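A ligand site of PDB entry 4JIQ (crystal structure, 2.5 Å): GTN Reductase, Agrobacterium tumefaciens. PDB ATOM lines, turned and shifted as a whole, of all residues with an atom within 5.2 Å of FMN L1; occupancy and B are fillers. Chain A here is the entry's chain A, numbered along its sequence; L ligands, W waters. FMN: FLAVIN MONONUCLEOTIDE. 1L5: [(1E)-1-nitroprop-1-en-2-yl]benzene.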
ATOM      1  N   ALA A  22     -25.298  10.734 -24.157  1.00  0.00           N
ATOM      2  CA  ALA A  22     -24.794  12.063 -23.859  1.00  0.00           C
ATOM      3  C   ALA A  22     -23.921  12.021 -22.601  1.00  0.00           C
ATOM      4  O   ALA A  22     -24.088  11.137 -21.764  1.00  0.00           O
ATOM      5  CB  ALA A  22     -25.943  13.042 -23.698  1.00  0.00           C
ATOM      6  N   PRO A  23     -22.985  12.968 -22.472  1.00  0.00           N
ATOM      7  CA  PRO A  23     -22.185  13.059 -21.252  1.00  0.00           C
ATOM      8  C   PRO A  23     -23.036  13.474 -20.058  1.00  0.00           C
ATOM      9  O   PRO A  23     -23.794  14.445 -20.160  1.00  0.00           O
ATOM     10  CB  PRO A  23     -21.144  14.144 -21.584  1.00  0.00           C
ATOM     11  CG  PRO A  23     -21.758  14.936 -22.687  1.00  0.00           C
ATOM     12  CD  PRO A  23     -22.570  13.965 -23.488  1.00  0.00           C
ATOM     13  N   LEU A  24     -22.911  12.743 -18.957  1.00  0.00           N
ATOM     14  CA  LEU A  24     -23.743  12.970 -17.780  1.00  0.00           C
ATOM     15  C   LEU A  24     -22.942  12.855 -16.486  1.00  0.00           C
ATOM     16  O   LEU A  24     -22.607  11.753 -16.061  1.00  0.00           O
ATOM     17  CB  LEU A  24     -24.885  11.958 -17.733  1.00  0.00           C
ATOM     18  CG  LEU A  24     -25.849  11.944 -18.910  1.00  0.00           C
ATOM     19  CD1 LEU A  24     -26.359  10.542 -19.148  1.00  0.00           C
ATOM     20  CD2 LEU A  24     -27.007  12.894 -18.640  1.00  0.00           C
ATOM     21  N   THR A  25     -22.636  13.999 -15.879  1.00  0.00           N
ATOM     22  CA  THR A  25     -21.972  14.020 -14.581  1.00  0.00           C
ATOM     23  C   THR A  25     -22.875  13.428 -13.505  1.00  0.00           C
ATOM     24  O   THR A  25     -24.019  13.838 -13.365  1.00  0.00           O
ATOM     25  CB  THR A  25     -21.590  15.455 -14.179  1.00  0.00           C
ATOM     26  OG1 THR A  25     -20.499  15.901 -14.988  1.00  0.00           O
ATOM     27  CG2 THR A  25     -21.187  15.521 -12.708  1.00  0.00           C
ATOM     28  N   ARG A  26     -22.365  12.453 -12.748  1.00  0.00           N
ATOM     29  CA  ARG A  26     -23.165  11.799 -11.714  1.00  0.00           C
ATOM     30  C   ARG A  26     -22.608  12.039 -10.321  1.00  0.00           C
ATOM     31  O   ARG A  26     -23.284  11.766  -9.322  1.00  0.00           O
ATOM     32  CB  ARG A  26     -23.268  10.297 -11.980  1.00  0.00           C
ATOM     33  CG  ARG A  26     -23.605   9.945 -13.416  1.00  0.00           C
ATOM     34  CD  ARG A  26     -24.937  10.541 -13.827  1.00  0.00           C
ATOM     35  NE  ARG A  26     -25.971  10.230 -12.836  1.00  0.00           N
ATOM     36  CZ  ARG A  26     -26.723   9.135 -12.878  1.00  0.00           C
ATOM     37  NH1 ARG A  26     -27.634   8.928 -11.935  1.00  0.00           N
ATOM     38  NH2 ARG A  26     -26.568   8.242 -13.847  1.00  0.00           N
ATOM     39  N   GLU A  54     -19.027  11.175 -18.700  1.00  0.00           N
ATOM     40  CA  GLU A  54     -19.248  12.410 -17.979  1.00  0.00           C
ATOM     41  C   GLU A  54     -18.004  13.277 -18.094  1.00  0.00           C
ATOM     42  O   GLU A  54     -16.910  12.765 -18.350  1.00  0.00           O
ATOM     43  CB  GLU A  54     -19.536  12.104 -16.509  1.00  0.00           C
ATOM     44  CG  GLU A  54     -18.407  11.341 -15.821  1.00  0.00           C
ATOM     45  CD  GLU A  54     -18.841  10.722 -14.511  1.00  0.00           C
ATOM     46  OE1 GLU A  54     -19.197  11.480 -13.589  1.00  0.00           O
ATOM     47  OE2 GLU A  54     -18.820   9.475 -14.409  1.00  0.00           O
ATOM     48  N   GLY A  55     -18.167  14.584 -17.923  1.00  0.00           N
ATOM     49  CA  GLY A  55     -17.068  15.520 -17.998  1.00  0.00           C
ATOM     50  C   GLY A  55     -15.920  15.114 -17.089  1.00  0.00           C
ATOM     51  O   GLY A  55     -16.103  14.884 -15.894  1.00  0.00           O
ATOM     52  N   GLN A  97     -14.873  12.818 -22.360  1.00  0.00           N
ATOM     53  CA  GLN A  97     -15.132  14.248 -22.485  1.00  0.00           C
ATOM     54  C   GLN A  97     -14.151  15.013 -21.593  1.00  0.00           C
ATOM     55  O   GLN A  97     -14.380  15.168 -20.394  1.00  0.00           O
ATOM     56  CB  GLN A  97     -16.570  14.599 -22.108  1.00  0.00           C
ATOM     57  CG  GLN A  97     -17.043  15.923 -22.699  1.00  0.00           C
ATOM     58  CD  GLN A  97     -18.284  16.484 -22.023  1.00  0.00           C
ATOM     59  OE1 GLN A  97     -18.467  16.334 -20.816  1.00  0.00           O
ATOM     60  NE2 GLN A  97     -19.139  17.124 -22.802  1.00  0.00           N
ATOM     61  N   HIS A 178     -14.764  19.444 -24.382  1.00  0.00           N
ATOM     62  CA  HIS A 178     -15.915  20.118 -23.778  1.00  0.00           C
ATOM     63  C   HIS A 178     -15.821  21.624 -23.991  1.00  0.00           C
ATOM     64  O   HIS A 178     -15.040  22.306 -23.324  1.00  0.00           O
ATOM     65  CB  HIS A 178     -16.025  19.785 -22.291  1.00  0.00           C
ATOM     66  CG  HIS A 178     -17.344  20.132 -21.686  1.00  0.00           C
ATOM     67  ND1 HIS A 178     -17.737  19.693 -20.436  1.00  0.00           N
ATOM     68  CD2 HIS A 178     -18.376  20.889 -22.154  1.00  0.00           C
ATOM     69  CE1 HIS A 178     -18.944  20.155 -20.172  1.00  0.00           C
ATOM     70  NE2 HIS A 178     -19.352  20.890 -21.192  1.00  0.00           N
ATOM     71  N   ASN A 181     -21.841  24.719 -22.418  1.00  0.00           N
ATOM     72  CA  ASN A 181     -22.443  24.966 -21.103  1.00  0.00           C
ATOM     73  C   ASN A 181     -21.710  25.957 -20.207  1.00  0.00           C
ATOM     74  O   ASN A 181     -21.721  25.838 -18.981  1.00  0.00           O
ATOM     75  CB  ASN A 181     -22.660  23.644 -20.354  1.00  0.00           C
ATOM     76  CG  ASN A 181     -23.500  22.664 -21.146  1.00  0.00           C
ATOM     77  OD1 ASN A 181     -24.214  23.059 -22.079  1.00  0.00           O
ATOM     78  ND2 ASN A 181     -23.445  21.400 -20.786  1.00  0.00           N
ATOM     79  N   ARG A 230     -17.910  19.377 -28.293  1.00  0.00           N
ATOM     80  CA  ARG A 230     -19.294  19.665 -27.945  1.00  0.00           C
ATOM     81  C   ARG A 230     -19.519  21.176 -27.877  1.00  0.00           C
ATOM     82  O   ARG A 230     -18.762  21.903 -27.249  1.00  0.00           O
ATOM     83  CB  ARG A 230     -19.646  19.004 -26.617  1.00  0.00           C
ATOM     84  CG  ARG A 230     -21.096  19.148 -26.196  1.00  0.00           C
ATOM     85  CD  ARG A 230     -21.366  18.323 -24.961  1.00  0.00           C
ATOM     86  NE  ARG A 230     -22.728  18.461 -24.443  1.00  0.00           N
ATOM     87  CZ  ARG A 230     -23.735  17.666 -24.779  1.00  0.00           C
ATOM     88  NH1 ARG A 230     -23.537  16.700 -25.638  1.00  0.00           N
ATOM     89  NH2 ARG A 230     -24.938  17.857 -24.269  1.00  0.00           N
ATOM     90  N   VAL A 267     -25.593  20.925 -28.784  1.00  0.00           N
ATOM     91  CA  VAL A 267     -26.744  21.061 -27.891  1.00  0.00           C
ATOM     92  C   VAL A 267     -27.725  22.072 -28.471  1.00  0.00           C
ATOM     93  O   VAL A 267     -27.443  23.265 -28.533  1.00  0.00           O
ATOM     94  CB  VAL A 267     -26.316  21.554 -26.497  1.00  0.00           C
ATOM     95  CG1 VAL A 267     -27.529  21.655 -25.584  1.00  0.00           C
ATOM     96  CG2 VAL A 267     -25.272  20.630 -25.906  1.00  0.00           C
ATOM     97  N   THR A 271     -29.672  24.060 -22.452  1.00  0.00           N
ATOM     98  CA  THR A 271     -29.351  22.747 -21.902  1.00  0.00           C
ATOM     99  C   THR A 271     -30.317  22.413 -20.774  1.00  0.00           C
ATOM    100  O   THR A 271     -30.359  23.102 -19.759  1.00  0.00           O
ATOM    101  CB  THR A 271     -27.912  22.682 -21.372  1.00  0.00           C
ATOM    102  OG1 THR A 271     -26.999  22.997 -22.432  1.00  0.00           O
ATOM    103  CG2 THR A 271     -27.604  21.294 -20.835  1.00  0.00           C
ATOM    104  N   GLY A 272     -31.097  21.344 -20.960  1.00  0.00           N
ATOM    105  CA  GLY A 272     -32.119  20.977 -20.000  1.00  0.00           C
ATOM    106  C   GLY A 272     -33.201  22.036 -19.962  1.00  0.00           C
ATOM    107  O   GLY A 272     -33.886  22.221 -18.954  1.00  0.00           O
ATOM    108  N   ASN A 305     -28.560  16.903 -29.867  1.00  0.00           N
ATOM    109  CA  ASN A 305     -28.971  16.605 -28.503  1.00  0.00           C
ATOM    110  C   ASN A 305     -29.998  17.607 -27.982  1.00  0.00           C
ATOM    111  O   ASN A 305     -30.084  18.731 -28.493  1.00  0.00           O
ATOM    112  CB  ASN A 305     -27.750  16.579 -27.587  1.00  0.00           C
ATOM    113  CG  ASN A 305     -28.123  16.519 -26.114  1.00  0.00           C
ATOM    114  OD1 ASN A 305     -28.064  17.533 -25.412  1.00  0.00           O
ATOM    115  ND2 ASN A 305     -28.548  15.346 -25.655  1.00  0.00           N
ATOM    116  N   ASN A 306     -30.781  17.156 -26.998  1.00  0.00           N
ATOM    117  CA  ASN A 306     -31.689  17.964 -26.158  1.00  0.00           C
ATOM    118  C   ASN A 306     -33.164  17.868 -26.524  1.00  0.00           C
ATOM    119  O   ASN A 306     -33.616  18.489 -27.486  1.00  0.00           O
ATOM    120  CB  ASN A 306     -31.240  19.433 -26.043  1.00  0.00           C
ATOM    121  CG  ASN A 306     -31.982  20.188 -24.957  1.00  0.00           C
ATOM    122  OD1 ASN A 306     -32.368  19.609 -23.944  1.00  0.00           O
ATOM    123  ND2 ASN A 306     -32.188  21.478 -25.173  1.00  0.00           N
ATOM    124  N   GLY A 307     -33.899  17.077 -25.749  1.00  0.00           N
ATOM    125  CA  GLY A 307     -35.344  17.007 -25.875  1.00  0.00           C
ATOM    126  C   GLY A 307     -35.834  16.024 -26.933  1.00  0.00           C
ATOM    127  O   GLY A 307     -36.987  16.091 -27.350  1.00  0.00           O
ATOM    128  N   TYR A 308     -34.953  15.125 -27.357  1.00  0.00           N
ATOM    129  CA  TYR A 308     -35.303  14.127 -28.366  1.00  0.00           C
ATOM    130  C   TYR A 308     -36.072  12.949 -27.775  1.00  0.00           C
ATOM    131  O   TYR A 308     -35.716  12.419 -26.720  1.00  0.00           O
ATOM    132  CB  TYR A 308     -34.051  13.619 -29.082  1.00  0.00           C
ATOM    133  CG  TYR A 308     -33.544  14.540 -30.173  1.00  0.00           C
ATOM    134  CD1 TYR A 308     -34.076  14.489 -31.454  1.00  0.00           C
ATOM    135  CD2 TYR A 308     -32.539  15.461 -29.921  1.00  0.00           C
ATOM    136  CE1 TYR A 308     -33.625  15.330 -32.457  1.00  0.00           C
ATOM    137  CE2 TYR A 308     -32.072  16.309 -30.911  1.00  0.00           C
ATOM    138  CZ  TYR A 308     -32.622  16.235 -32.180  1.00  0.00           C
ATOM    139  OH  TYR A 308     -32.166  17.078 -33.162  1.00  0.00           O
ATOM    140  N   ALA A 326     -28.127  12.099 -29.476  1.00  0.00           N
ATOM    141  CA  ALA A 326     -27.633  11.803 -28.135  1.00  0.00           C
ATOM    142  C   ALA A 326     -28.708  12.043 -27.068  1.00  0.00           C
ATOM    143  O   ALA A 326     -29.290  13.121 -26.987  1.00  0.00           O
ATOM    144  CB  ALA A 326     -26.381  12.609 -27.832  1.00  0.00           C
ATOM    145  N   PHE A 327     -28.937  11.015 -26.252  1.00  0.00           N
ATOM    146  CA  PHE A 327     -29.913  11.084 -25.175  1.00  0.00           C
ATOM    147  C   PHE A 327     -29.199  11.147 -23.834  1.00  0.00           C
ATOM    148  O   PHE A 327     -28.241  10.406 -23.603  1.00  0.00           O
ATOM    149  CB  PHE A 327     -30.832   9.860 -25.214  1.00  0.00           C
ATOM    150  CG  PHE A 327     -31.490   9.631 -26.547  1.00  0.00           C
ATOM    151  CD1 PHE A 327     -30.876   8.854 -27.517  1.00  0.00           C
ATOM    152  CD2 PHE A 327     -32.732  10.186 -26.817  1.00  0.00           C
ATOM    153  CE1 PHE A 327     -31.481   8.637 -28.735  1.00  0.00           C
ATOM    154  CE2 PHE A 327     -33.343   9.970 -28.043  1.00  0.00           C
ATOM    155  CZ  PHE A 327     -32.717   9.190 -28.998  1.00  0.00           C
ATOM    156  N   GLY A 328     -29.651  12.036 -22.957  1.00  0.00           N
ATOM    157  CA  GLY A 328     -29.046  12.184 -21.644  1.00  0.00           C
ATOM    158  C   GLY A 328     -29.862  11.505 -20.547  1.00  0.00           C
ATOM    159  O   GLY A 328     -29.488  10.444 -20.058  1.00  0.00           O
ATOM    160  N   LYS A 329     -30.972  12.126 -20.170  1.00  0.00           N
ATOM    161  CA  LYS A 329     -31.821  11.612 -19.088  1.00  0.00           C
ATOM    162  C   LYS A 329     -32.417  10.246 -19.379  1.00  0.00           C
ATOM    163  O   LYS A 329     -32.684   9.475 -18.467  1.00  0.00           O
ATOM    164  CB  LYS A 329     -32.918  12.619 -18.743  1.00  0.00           C
ATOM    165  CG  LYS A 329     -32.426  13.844 -18.004  1.00  0.00           C
ATOM    166  CD  LYS A 329     -33.578  14.712 -17.529  1.00  0.00           C
ATOM    167  CE  LYS A 329     -33.572  16.056 -18.230  1.00  0.00           C
ATOM    168  NZ  LYS A 329     -33.678  15.907 -19.712  1.00  0.00           N
ATOM    169  N   ALA A 330     -32.630   9.939 -20.664  1.00  0.00           N
ATOM    170  CA  ALA A 330     -33.195   8.660 -21.060  1.00  0.00           C
ATOM    171  C   ALA A 330     -32.205   7.512 -20.863  1.00  0.00           C
ATOM    172  O   ALA A 330     -32.603   6.385 -20.550  1.00  0.00           O
ATOM    173  CB  ALA A 330     -33.684   8.712 -22.507  1.00  0.00           C
ATOM    174  N   ILE A 332     -29.939   7.590 -18.536  1.00  0.00           N
ATOM    175  CA  ILE A 332     -29.845   7.451 -17.086  1.00  0.00           C
ATOM    176  C   ILE A 332     -30.864   6.419 -16.619  1.00  0.00           C
ATOM    177  O   ILE A 332     -30.546   5.502 -15.865  1.00  0.00           O
ATOM    178  CB  ILE A 332     -30.108   8.791 -16.367  1.00  0.00           C
ATOM    179  CG1 ILE A 332     -28.989   9.793 -16.673  1.00  0.00           C
ATOM    180  CG2 ILE A 332     -30.252   8.585 -14.872  1.00  0.00           C
ATOM    181  CD1 ILE A 332     -29.171  11.137 -15.982  1.00  0.00           C
ATOM    182  N   PHE A 355     -29.888  11.987  -9.388  1.00  0.00           N
ATOM    183  CA  PHE A 355     -29.018  12.355 -10.496  1.00  0.00           C
ATOM    184  C   PHE A 355     -27.576  12.599 -10.068  1.00  0.00           C
ATOM    185  O   PHE A 355     -26.634  12.182 -10.760  1.00  0.00           O
ATOM    186  CB  PHE A 355     -29.544  13.584 -11.228  1.00  0.00           C
ATOM    187  CG  PHE A 355     -30.617  13.287 -12.237  1.00  0.00           C
ATOM    188  CD1 PHE A 355     -31.198  12.036 -12.314  1.00  0.00           C
ATOM    189  CD2 PHE A 355     -31.031  14.269 -13.137  1.00  0.00           C
ATOM    190  CE1 PHE A 355     -32.182  11.752 -13.237  1.00  0.00           C
ATOM    191  CE2 PHE A 355     -32.018  13.995 -14.070  1.00  0.00           C
ATOM    192  CZ  PHE A 355     -32.593  12.746 -14.126  1.00  0.00           C
ATOM    193  N   TYR A 356     -27.385  13.270  -8.935  1.00  0.00           N
ATOM    194  CA  TYR A 356     -26.052  13.635  -8.462  1.00  0.00           C
ATOM    195  C   TYR A 356     -25.771  13.063  -7.074  1.00  0.00           C
ATOM    196  O   TYR A 356     -26.626  13.095  -6.196  1.00  0.00           O
ATOM    197  CB  TYR A 356     -25.875  15.149  -8.415  1.00  0.00           C
ATOM    198  CG  TYR A 356     -26.286  15.867  -9.685  1.00  0.00           C
ATOM    199  CD1 TYR A 356     -25.441  15.905 -10.781  1.00  0.00           C
ATOM    200  CD2 TYR A 356     -27.509  16.517  -9.773  1.00  0.00           C
ATOM    201  CE1 TYR A 356     -25.805  16.559 -11.942  1.00  0.00           C
ATOM    202  CE2 TYR A 356     -27.880  17.175 -10.928  1.00  0.00           C
ATOM    203  CZ  TYR A 356     -27.030  17.193 -12.005  1.00  0.00           C
ATOM    204  OH  TYR A 356     -27.398  17.838 -13.165  1.00  0.00           O
HETATM  205  N1  FMN L   1     -23.561  17.897 -20.506  1.00  0.00           N
HETATM  206  C2  FMN L   1     -22.203  17.863 -20.743  1.00  0.00           C
HETATM  207  O2  FMN L   1     -21.738  18.325 -21.787  1.00  0.00           O
HETATM  208  N3  FMN L   1     -21.350  17.297 -19.821  1.00  0.00           N
HETATM  209  C4  FMN L   1     -21.845  16.775 -18.642  1.00  0.00           C
HETATM  210  O4  FMN L   1     -21.062  16.270 -17.836  1.00  0.00           O
HETATM  211  C4A FMN L   1     -23.213  16.830 -18.381  1.00  0.00           C
HETATM  212  N5  FMN L   1     -23.747  16.321 -17.220  1.00  0.00           N
HETATM  213  C5A FMN L   1     -25.116  16.239 -17.031  1.00  0.00           C
HETATM  214  C6  FMN L   1     -25.621  15.602 -15.900  1.00  0.00           C
HETATM  215  C7  FMN L   1     -27.000  15.513 -15.716  1.00  0.00           C
HETATM  216  C7M FMN L   1     -27.537  14.818 -14.501  1.00  0.00           C
HETATM  217  C8  FMN L   1     -27.867  16.059 -16.656  1.00  0.00           C
HETATM  218  C8M FMN L   1     -29.350  15.962 -16.451  1.00  0.00           C
HETATM  219  C9  FMN L   1     -27.351  16.704 -17.781  1.00  0.00           C
HETATM  220  C9A FMN L   1     -25.976  16.782 -17.977  1.00  0.00           C
HETATM  221  N10 FMN L   1     -25.434  17.391 -19.116  1.00  0.00           N
HETATM  222  C10 FMN L   1     -24.059  17.389 -19.323  1.00  0.00           C
HETATM  223  C1' FMN L   1     -26.284  17.703 -20.301  1.00  0.00           C
HETATM  224  C2' FMN L   1     -26.680  16.444 -21.060  1.00  0.00           C
HETATM  225  O2' FMN L   1     -25.534  15.847 -21.622  1.00  0.00           O
HETATM  226  C3' FMN L   1     -27.651  16.776 -22.180  1.00  0.00           C
HETATM  227  O3' FMN L   1     -27.229  17.938 -22.862  1.00  0.00           O
HETATM  228  C4' FMN L   1     -29.091  16.991 -21.716  1.00  0.00           C
HETATM  229  O4' FMN L   1     -29.212  17.902 -20.641  1.00  0.00           O
HETATM  230  C5' FMN L   1     -29.711  15.653 -21.327  1.00  0.00           C
HETATM  231  O5' FMN L   1     -31.098  15.761 -21.540  1.00  0.00           O
HETATM  232  P   FMN L   1     -31.695  15.230 -22.930  1.00  0.00           P
HETATM  233  O1P FMN L   1     -31.719  13.724 -22.947  1.00  0.00           O
HETATM  234  O2P FMN L   1     -30.835  15.740 -24.062  1.00  0.00           O
HETATM  235  O3P FMN L   1     -33.100  15.761 -23.054  1.00  0.00           O
HETATM  236  C1  1L5 L   2     -22.487  19.619 -15.680  1.00  0.00           C
HETATM  237  C2  1L5 L   2     -23.038  19.728 -14.283  1.00  0.00           C
HETATM  238  C3  1L5 L   2     -24.301  20.280 -14.076  1.00  0.00           C
HETATM  239  C4  1L5 L   2     -24.838  20.393 -12.795  1.00  0.00           C
HETATM  240  C5  1L5 L   2     -24.113  19.938 -11.697  1.00  0.00           C
HETATM  241  C6  1L5 L   2     -22.855  19.388 -11.913  1.00  0.00           C
HETATM  242  C7  1L5 L   2     -22.318  19.275 -13.193  1.00  0.00           C
HETATM  243  C8  1L5 L   2     -23.071  20.353 -16.632  1.00  0.00           C
HETATM  244  O1  1L5 L   2     -23.648  20.253 -18.671  1.00  0.00           O
HETATM  245  N   1L5 L   2     -22.752  20.342 -17.859  1.00  0.00           N
HETATM  246  O   1L5 L   2     -21.445  20.452 -18.360  1.00  0.00           O
HETATM  247  C   1L5 L   2     -21.313  18.748 -16.016  1.00  0.00           C
HETATM  248  O   HOH W   1     -31.883  14.333 -26.763  1.00  0.00           O
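N of Gly 307 is in hydrogen-bond range of O3P of FMN L1, 3.1 Å away.
An oxygen (O2') of FMN L1 is in hydrogen-bond range of the backbone carbonyl oxygen of Pro 23 (2.7 Å).
O1P of FMN L1 sits at hydrogen-bond distance from N of Gly 328 (2.7 Å).
NZ of Lys 329 lies within salt-bridge range of O3P of FMN L1.
The backbone NH (N) of Lys 329 sits at hydrogen-bond distance from an oxygen (O1P) of FMN L1 (3.3 Å).
A nitrogen (N5) of FMN L1 sits at hydrogen-bond distance from the backbone NH (N) of Thr 25, at 2.9 Å.
The backbone NH (N) of Gly 55 lies within hydrogen-bond range of an oxygen (O4) of FMN L1.
The side-chain amide oxygen (OD1) of Asn 305 sits at hydrogen-bond distance from an oxygen (O3') of FMN L1, 2.7 Å away.
The side-chain amide nitrogen of Gln 97 sits at hydrogen-bond distance from an oxygen (O2) of FMN L1 (3.0 Å).
An oxygen (O3') of FMN L1 lies within hydrogen-bond range of the guanidinium group (NH2) of Arg 230, 2.7 Å away.
O2P of FMN L1 lies close to N of Asn 306 (3.3 Å).
OG1 of Thr 25 is in hydrogen-bond range of O4 of FMN L1 (2.9 Å).
ND2 of Asn 181 sits at hydrogen-bond distance from O1 of 1L5 L2 (2.4 Å).
N3 of FMN L1 lies within hydrogen-bond range of O of 1L5 L2 (3.5 Å).
The side-chain amide nitrogen (ND2) of Asn 305 is in hydrogen-bond range of the backbone carbonyl oxygen (O) of Ala 326.
The guanidinium group (NH2) of Arg 230 sits at hydrogen-bond distance from the side-chain amide oxygen (OD1) of Asn 305 (3.3 Å).
The backbone NH (N) of Ala 22 is in hydrogen-bond range of the backbone carbonyl oxygen (O) of Phe 327 (3.0 Å).
OG1 of Thr 271 is in hydrogen-bond range of OD1 of Asn 181 (2.8 Å).
The side-chain amide oxygen (OE1) of Gln 97 lies close to the backbone NH (N) of Gly 55 (3.4 Å).
The side-chain amide oxygen (OE1) of Gln 97 is in hydrogen-bond range of a ring nitrogen (ND1) of His 178 (3.5 Å).
O of Phe 355 is in hydrogen-bond range of NE of Arg 26 (2.9 Å).
Ala 22 touches FMN L1 (CB to O2', 3.5 Å).
Leu 24 touches FMN L1 (CA to N5, 3.4 Å).
His 178 touches FMN L1 (NE2 to O2, 3.6 Å).
Asn 181 touches FMN L1 (ND2 to N1, 3.5 Å).
Thr 271 touches FMN L1.
Gly 272 touches FMN L1 (N to O4', 3.9 Å).
Phe 327 touches FMN L1.
Phe 355 touches FMN L1.
Tyr 356 touches FMN L1.
Hydrophobic or aromatic side chains that line FMN L1: Ala 22, Pro 23, Leu 24, His 178, Phe 355 and Tyr 356.
Of the 26 residues printed, 19 come within 4 Å of FMN L1.
Water W1 lies within hydrogen-bond range of the backbone carbonyl oxygen (O) of Ala 326 (2.9 Å), the backbone NH (N) of Asn 306 (3.0 Å), an oxygen (O2P) of FMN L1 (3.2 Å) and the backbone NH (N) of Tyr 308 (3.2 Å).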
